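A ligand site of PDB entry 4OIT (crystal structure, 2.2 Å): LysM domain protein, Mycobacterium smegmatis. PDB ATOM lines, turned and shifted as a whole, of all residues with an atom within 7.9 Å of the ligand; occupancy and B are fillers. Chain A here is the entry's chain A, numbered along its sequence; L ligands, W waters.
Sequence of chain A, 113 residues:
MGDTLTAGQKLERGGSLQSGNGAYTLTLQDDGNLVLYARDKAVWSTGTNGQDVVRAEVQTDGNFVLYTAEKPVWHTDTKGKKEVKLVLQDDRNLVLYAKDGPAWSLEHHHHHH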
ATOM      1  N   GLN A  29      -5.176 -10.737 -15.658  1.00  0.00           N
ATOM      2  CA  GLN A  29      -6.322 -11.467 -15.128  1.00  0.00           C
ATOM      3  C   GLN A  29      -7.526 -11.450 -16.071  1.00  0.00           C
ATOM      4  O   GLN A  29      -7.587 -10.641 -16.999  1.00  0.00           O
ATOM      5  CB  GLN A  29      -6.721 -10.889 -13.766  1.00  0.00           C
ATOM      6  CG  GLN A  29      -5.564 -10.773 -12.783  1.00  0.00           C
ATOM      7  CD  GLN A  29      -5.997 -10.365 -11.377  1.00  0.00           C
ATOM      8  OE1 GLN A  29      -5.446 -10.856 -10.404  1.00  0.00           O
ATOM      9  NE2 GLN A  29      -6.974  -9.460 -11.276  1.00  0.00           N
ATOM     10  N   ASP A  31     -10.524 -10.590 -15.255  1.00  0.00           N
ATOM     11  CA  ASP A  31     -11.308  -9.368 -15.015  1.00  0.00           C
ATOM     12  C   ASP A  31     -10.772  -8.167 -15.800  1.00  0.00           C
ATOM     13  O   ASP A  31     -11.366  -7.084 -15.771  1.00  0.00           O
ATOM     14  CB  ASP A  31     -11.374  -9.041 -13.517  1.00  0.00           C
ATOM     15  CG  ASP A  31     -10.048  -8.534 -12.946  1.00  0.00           C
ATOM     16  OD1 ASP A  31      -9.024  -8.525 -13.666  1.00  0.00           O
ATOM     17  OD2 ASP A  31     -10.032  -8.162 -11.765  1.00  0.00           O
ATOM     18  N   GLY A  32      -9.646  -8.343 -16.486  1.00  0.00           N
ATOM     19  CA  GLY A  32      -9.056  -7.299 -17.339  1.00  0.00           C
ATOM     20  C   GLY A  32      -7.846  -6.595 -16.747  1.00  0.00           C
ATOM     21  O   GLY A  32      -7.131  -5.891 -17.452  1.00  0.00           O
ATOM     22  N   ASN A  33      -7.615  -6.786 -15.457  1.00  0.00           N
ATOM     23  CA  ASN A  33      -6.551  -6.075 -14.753  1.00  0.00           C
ATOM     24  C   ASN A  33      -5.202  -6.778 -14.875  1.00  0.00           C
ATOM     25  O   ASN A  33      -5.105  -7.997 -14.697  1.00  0.00           O
ATOM     26  CB  ASN A  33      -6.913  -5.895 -13.282  1.00  0.00           C
ATOM     27  CG  ASN A  33      -6.282  -4.659 -12.664  1.00  0.00           C
ATOM     28  OD1 ASN A  33      -5.605  -3.879 -13.332  1.00  0.00           O
ATOM     29  ND2 ASN A  33      -6.511  -4.476 -11.370  1.00  0.00           N
ATOM     30  N   LEU A  34      -4.164  -6.011 -15.189  1.00  0.00           N
ATOM     31  CA  LEU A  34      -2.787  -6.489 -15.114  1.00  0.00           C
ATOM     32  C   LEU A  34      -2.278  -6.142 -13.731  1.00  0.00           C
ATOM     33  O   LEU A  34      -2.133  -4.967 -13.409  1.00  0.00           O
ATOM     34  CB  LEU A  34      -1.913  -5.821 -16.179  1.00  0.00           C
ATOM     35  CG  LEU A  34      -0.420  -6.197 -16.155  1.00  0.00           C
ATOM     36  CD1 LEU A  34      -0.222  -7.638 -16.627  1.00  0.00           C
ATOM     37  CD2 LEU A  34       0.391  -5.240 -17.004  1.00  0.00           C
ATOM     38  N   VAL A  35      -2.013  -7.172 -12.924  1.00  0.00           N
ATOM     39  CA  VAL A  35      -1.699  -6.976 -11.510  1.00  0.00           C
ATOM     40  C   VAL A  35      -0.330  -7.541 -11.157  1.00  0.00           C
ATOM     41  O   VAL A  35       0.054  -8.610 -11.646  1.00  0.00           O
ATOM     42  CB  VAL A  35      -2.745  -7.647 -10.593  1.00  0.00           C
ATOM     43  CG1 VAL A  35      -2.511  -7.261  -9.138  1.00  0.00           C
ATOM     44  CG2 VAL A  35      -4.154  -7.278 -11.016  1.00  0.00           C
ATOM     45  N   LEU A  36       0.392  -6.811 -10.311  1.00  0.00           N
ATOM     46  CA  LEU A  36       1.625  -7.292  -9.711  1.00  0.00           C
ATOM     47  C   LEU A  36       1.338  -7.719  -8.268  1.00  0.00           C
ATOM     48  O   LEU A  36       1.073  -6.869  -7.408  1.00  0.00           O
ATOM     49  CB  LEU A  36       2.700  -6.215  -9.747  1.00  0.00           C
ATOM     50  CG  LEU A  36       4.017  -6.537  -9.018  1.00  0.00           C
ATOM     51  CD1 LEU A  36       4.665  -7.793  -9.569  1.00  0.00           C
ATOM     52  CD2 LEU A  36       4.971  -5.352  -9.093  1.00  0.00           C
ATOM     53  N   TYR A  37       1.377  -9.022  -8.014  1.00  0.00           N
ATOM     54  CA  TYR A  37       1.228  -9.565  -6.672  1.00  0.00           C
ATOM     55  C   TYR A  37       2.580  -9.774  -6.023  1.00  0.00           C
ATOM     56  O   TYR A  37       3.415 -10.517  -6.546  1.00  0.00           O
ATOM     57  CB  TYR A  37       0.468 -10.888  -6.712  1.00  0.00           C
ATOM     58  CG  TYR A  37      -0.983 -10.720  -7.076  1.00  0.00           C
ATOM     59  CD1 TYR A  37      -1.912 -10.297  -6.131  1.00  0.00           C
ATOM     60  CD2 TYR A  37      -1.423 -10.981  -8.366  1.00  0.00           C
ATOM     61  CE1 TYR A  37      -3.247 -10.136  -6.463  1.00  0.00           C
ATOM     62  CE2 TYR A  37      -2.753 -10.831  -8.706  1.00  0.00           C
ATOM     63  CZ  TYR A  37      -3.665 -10.397  -7.752  1.00  0.00           C
ATOM     64  OH  TYR A  37      -4.982 -10.243  -8.089  1.00  0.00           O
ATOM     65  N   ASP A  40       1.353 -12.015  -0.438  1.00  0.00           N
ATOM     66  CA  ASP A  40      -0.105 -11.988  -0.225  1.00  0.00           C
ATOM     67  C   ASP A  40      -0.816 -10.848  -0.962  1.00  0.00           C
ATOM     68  O   ASP A  40      -1.903 -11.043  -1.505  1.00  0.00           O
ATOM     69  CB  ASP A  40      -0.438 -11.954   1.282  1.00  0.00           C
ATOM     70  CG  ASP A  40       0.174 -10.752   2.008  1.00  0.00           C
ATOM     71  OD1 ASP A  40      -0.069  -9.608   1.588  1.00  0.00           O
ATOM     72  OD2 ASP A  40       0.875 -10.969   3.019  1.00  0.00           O
ATOM     73  N   LYS A  41      -0.195  -9.677  -0.975  1.00  0.00           N
ATOM     74  CA  LYS A  41      -0.846  -8.440  -1.408  1.00  0.00           C
ATOM     75  C   LYS A  41      -0.589  -8.078  -2.869  1.00  0.00           C
ATOM     76  O   LYS A  41       0.474  -8.389  -3.417  1.00  0.00           O
ATOM     77  CB  LYS A  41      -0.407  -7.278  -0.517  1.00  0.00           C
ATOM     78  N   ALA A  42      -1.566  -7.421  -3.472  1.00  0.00           N
ATOM     79  CA  ALA A  42      -1.390  -6.758  -4.758  1.00  0.00           C
ATOM     80  C   ALA A  42      -0.791  -5.372  -4.498  1.00  0.00           C
ATOM     81  O   ALA A  42      -1.401  -4.549  -3.825  1.00  0.00           O
ATOM     82  CB  ALA A  42      -2.717  -6.631  -5.485  1.00  0.00           C
ATOM     83  N   VAL A  43       0.404  -5.133  -5.029  1.00  0.00           N
ATOM     84  CA  VAL A  43       1.126  -3.875  -4.780  1.00  0.00           C
ATOM     85  C   VAL A  43       0.852  -2.810  -5.852  1.00  0.00           C
ATOM     86  O   VAL A  43       1.030  -1.618  -5.602  1.00  0.00           O
ATOM     87  CB  VAL A  43       2.654  -4.089  -4.650  1.00  0.00           C
ATOM     88  CG1 VAL A  43       2.955  -4.907  -3.414  1.00  0.00           C
ATOM     89  CG2 VAL A  43       3.257  -4.727  -5.895  1.00  0.00           C
ATOM     90  N   TRP A  44       0.431  -3.257  -7.037  1.00  0.00           N
ATOM     91  CA  TRP A  44       0.161  -2.356  -8.145  1.00  0.00           C
ATOM     92  C   TRP A  44      -0.678  -3.032  -9.232  1.00  0.00           C
ATOM     93  O   TRP A  44      -0.624  -4.254  -9.393  1.00  0.00           O
ATOM     94  CB  TRP A  44       1.477  -1.852  -8.740  1.00  0.00           C
ATOM     95  CG  TRP A  44       1.336  -0.994  -9.971  1.00  0.00           C
ATOM     96  CD1 TRP A  44       1.136   0.354 -10.016  1.00  0.00           C
ATOM     97  CD2 TRP A  44       1.423  -1.438 -11.331  1.00  0.00           C
ATOM     98  NE1 TRP A  44       1.080   0.780 -11.329  1.00  0.00           N
ATOM     99  CE2 TRP A  44       1.251  -0.305 -12.154  1.00  0.00           C
ATOM    100  CE3 TRP A  44       1.620  -2.683 -11.938  1.00  0.00           C
ATOM    101  CZ2 TRP A  44       1.269  -0.373 -13.542  1.00  0.00           C
ATOM    102  CZ3 TRP A  44       1.647  -2.755 -13.328  1.00  0.00           C
ATOM    103  CH2 TRP A  44       1.469  -1.603 -14.114  1.00  0.00           C
ATOM    104  N   SER A  45      -1.441  -2.231  -9.954  1.00  0.00           N
ATOM    105  CA  SER A  45      -2.148  -2.706 -11.135  1.00  0.00           C
ATOM    106  C   SER A  45      -2.361  -1.584 -12.145  1.00  0.00           C
ATOM    107  O   SER A  45      -2.126  -0.415 -11.850  1.00  0.00           O
ATOM    108  CB  SER A  45      -3.489  -3.358 -10.758  1.00  0.00           C
ATOM    109  OG  SER A  45      -4.513  -2.401 -10.575  1.00  0.00           O
ATOM    110  N   THR A  46      -2.820  -1.958 -13.329  1.00  0.00           N
ATOM    111  CA  THR A  46      -3.132  -1.000 -14.388  1.00  0.00           C
ATOM    112  C   THR A  46      -4.525  -0.380 -14.225  1.00  0.00           C
ATOM    113  O   THR A  46      -4.866   0.556 -14.927  1.00  0.00           O
ATOM    114  CB  THR A  46      -3.049  -1.658 -15.782  1.00  0.00           C
ATOM    115  OG1 THR A  46      -3.888  -2.812 -15.830  1.00  0.00           O
ATOM    116  CG2 THR A  46      -1.617  -2.054 -16.095  1.00  0.00           C
ATOM    117  N   GLY A  47      -5.320  -0.900 -13.291  1.00  0.00           N
ATOM    118  CA  GLY A  47      -6.671  -0.414 -13.061  1.00  0.00           C
ATOM    119  C   GLY A  47      -7.610  -0.708 -14.219  1.00  0.00           C
ATOM    120  O   GLY A  47      -8.560   0.034 -14.454  1.00  0.00           O
ATOM    121  N   THR A  48      -7.343  -1.788 -14.932  1.00  0.00           N
ATOM    122  CA  THR A  48      -8.142  -2.174 -16.091  1.00  0.00           C
ATOM    123  C   THR A  48      -9.119  -3.307 -15.755  1.00  0.00           C
ATOM    124  O   THR A  48      -9.590  -4.010 -16.653  1.00  0.00           O
ATOM    125  CB  THR A  48      -7.249  -2.551 -17.295  1.00  0.00           C
ATOM    126  OG1 THR A  48      -6.210  -3.442 -16.871  1.00  0.00           O
ATOM    127  CG2 THR A  48      -6.600  -1.305 -17.882  1.00  0.00           C
ATOM    128  N   ASN A  49      -9.430  -3.468 -14.472  1.00  0.00           N
ATOM    129  CA  ASN A  49     -10.484  -4.396 -14.060  1.00  0.00           C
ATOM    130  C   ASN A  49     -11.840  -3.920 -14.569  1.00  0.00           C
ATOM    131  O   ASN A  49     -12.113  -2.721 -14.628  1.00  0.00           O
ATOM    132  CB  ASN A  49     -10.526  -4.614 -12.539  1.00  0.00           C
ATOM    133  CG  ASN A  49     -10.490  -3.321 -11.743  1.00  0.00           C
ATOM    134  OD1 ASN A  49      -9.626  -2.466 -11.965  1.00  0.00           O
ATOM    135  ND2 ASN A  49     -11.406  -3.176 -10.790  1.00  0.00           N
ATOM    136  N   GLY A  50     -12.691  -4.870 -14.974  1.00  0.00           N
ATOM    137  CA  GLY A  50     -13.988  -4.552 -15.574  1.00  0.00           C
ATOM    138  C   GLY A  50     -13.905  -4.199 -17.054  1.00  0.00           C
ATOM    139  O   GLY A  50     -14.916  -3.823 -17.663  1.00  0.00           O
HETATM  140  C1  LIG L   1      -9.020  -5.041  -8.161  1.00  0.00           C
HETATM  141  C2  LIG L   1      -9.171  -6.513  -8.571  1.00  0.00           C
HETATM  142  C3  LIG L   1      -8.145  -7.435  -7.929  1.00  0.00           C
HETATM  143  C4  LIG L   1      -6.750  -6.835  -8.016  1.00  0.00           C
HETATM  144  C5  LIG L   1      -6.738  -5.377  -7.567  1.00  0.00           C
HETATM  145  C6  LIG L   1      -5.368  -4.750  -7.793  1.00  0.00           C
HETATM  146  O1  LIG L   1      -9.429  -4.812  -6.825  1.00  0.00           O
HETATM  147  O2  LIG L   1      -8.996  -6.597  -9.969  1.00  0.00           O
HETATM  148  O3  LIG L   1      -8.130  -8.666  -8.623  1.00  0.00           O
HETATM  149  O4  LIG L   1      -5.895  -7.617  -7.222  1.00  0.00           O
HETATM  150  O5  LIG L   1      -7.674  -4.628  -8.324  1.00  0.00           O
HETATM  151  O6  LIG L   1      -5.222  -3.627  -6.953  1.00  0.00           O
HETATM  152  O   HOH W   1      -3.861  -3.179  -4.588  1.00  0.00           O
HETATM  153  O   HOH W   2      -8.450 -10.698  -6.132  1.00  0.00           O
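O2 of the ligand lies within hydrogen-bond range of OD2 of Asp 31 (2.6 Å). The side-chain hydroxyl (OH) of Tyr 37 lies within hydrogen-bond range of an oxygen (O4) of the ligand, 2.9 Å away. The side-chain amide nitrogen (NE2) of Gln 29 sits at hydrogen-bond distance from an oxygen (O3) of the ligand. An oxygen (O5) of the ligand is in hydrogen-bond range of the side-chain amide nitrogen (ND2) of Asn 33 (3.3 Å).
The side-chain amide nitrogen of Asn 33 lies within hydrogen-bond range of the side-chain hydroxyl of Ser 45. N of Gly 47 sits at hydrogen-bond distance from OD1 of Asn 33. The side-chain carboxylate (OD1) of Asp 31 is in hydrogen-bond range of the backbone NH (N) of Asn 33, at 2.9 Å. The side-chain amide oxygen (OD1) of Asn 33 is in hydrogen-bond range of the side-chain hydroxyl (OG1) of Thr 46 (3.2 Å). OD1 of Asn 33 sits at hydrogen-bond distance from N of Thr 48 (3.2 Å). N of Gly 47 lies within hydrogen-bond range of OG of Ser 45 (3.2 Å). OH of Tyr 37 is in hydrogen-bond range of OE1 of Gln 29, at 2.4 Å. The backbone carbonyl oxygen of Asp 31 lies within hydrogen-bond range of the backbone NH of Gly 50 (2.7 Å).
Val 35 touches the ligand. Ala 42 touches the ligand (CB to O4, 3.8 Å). OG of Ser 45 touches C6 of the ligand (3.7 Å). Asn 49 touches the ligand. Hydrophobic or aromatic side chains within 4 Å of the ligand: Val 35, Tyr 37 and Ala 42.
Water W1 lies within hydrogen-bond range of an oxygen (O6) of the ligand (2.8 Å) and the backbone carbonyl oxygen (O) of Ala 42 (2.9 Å).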
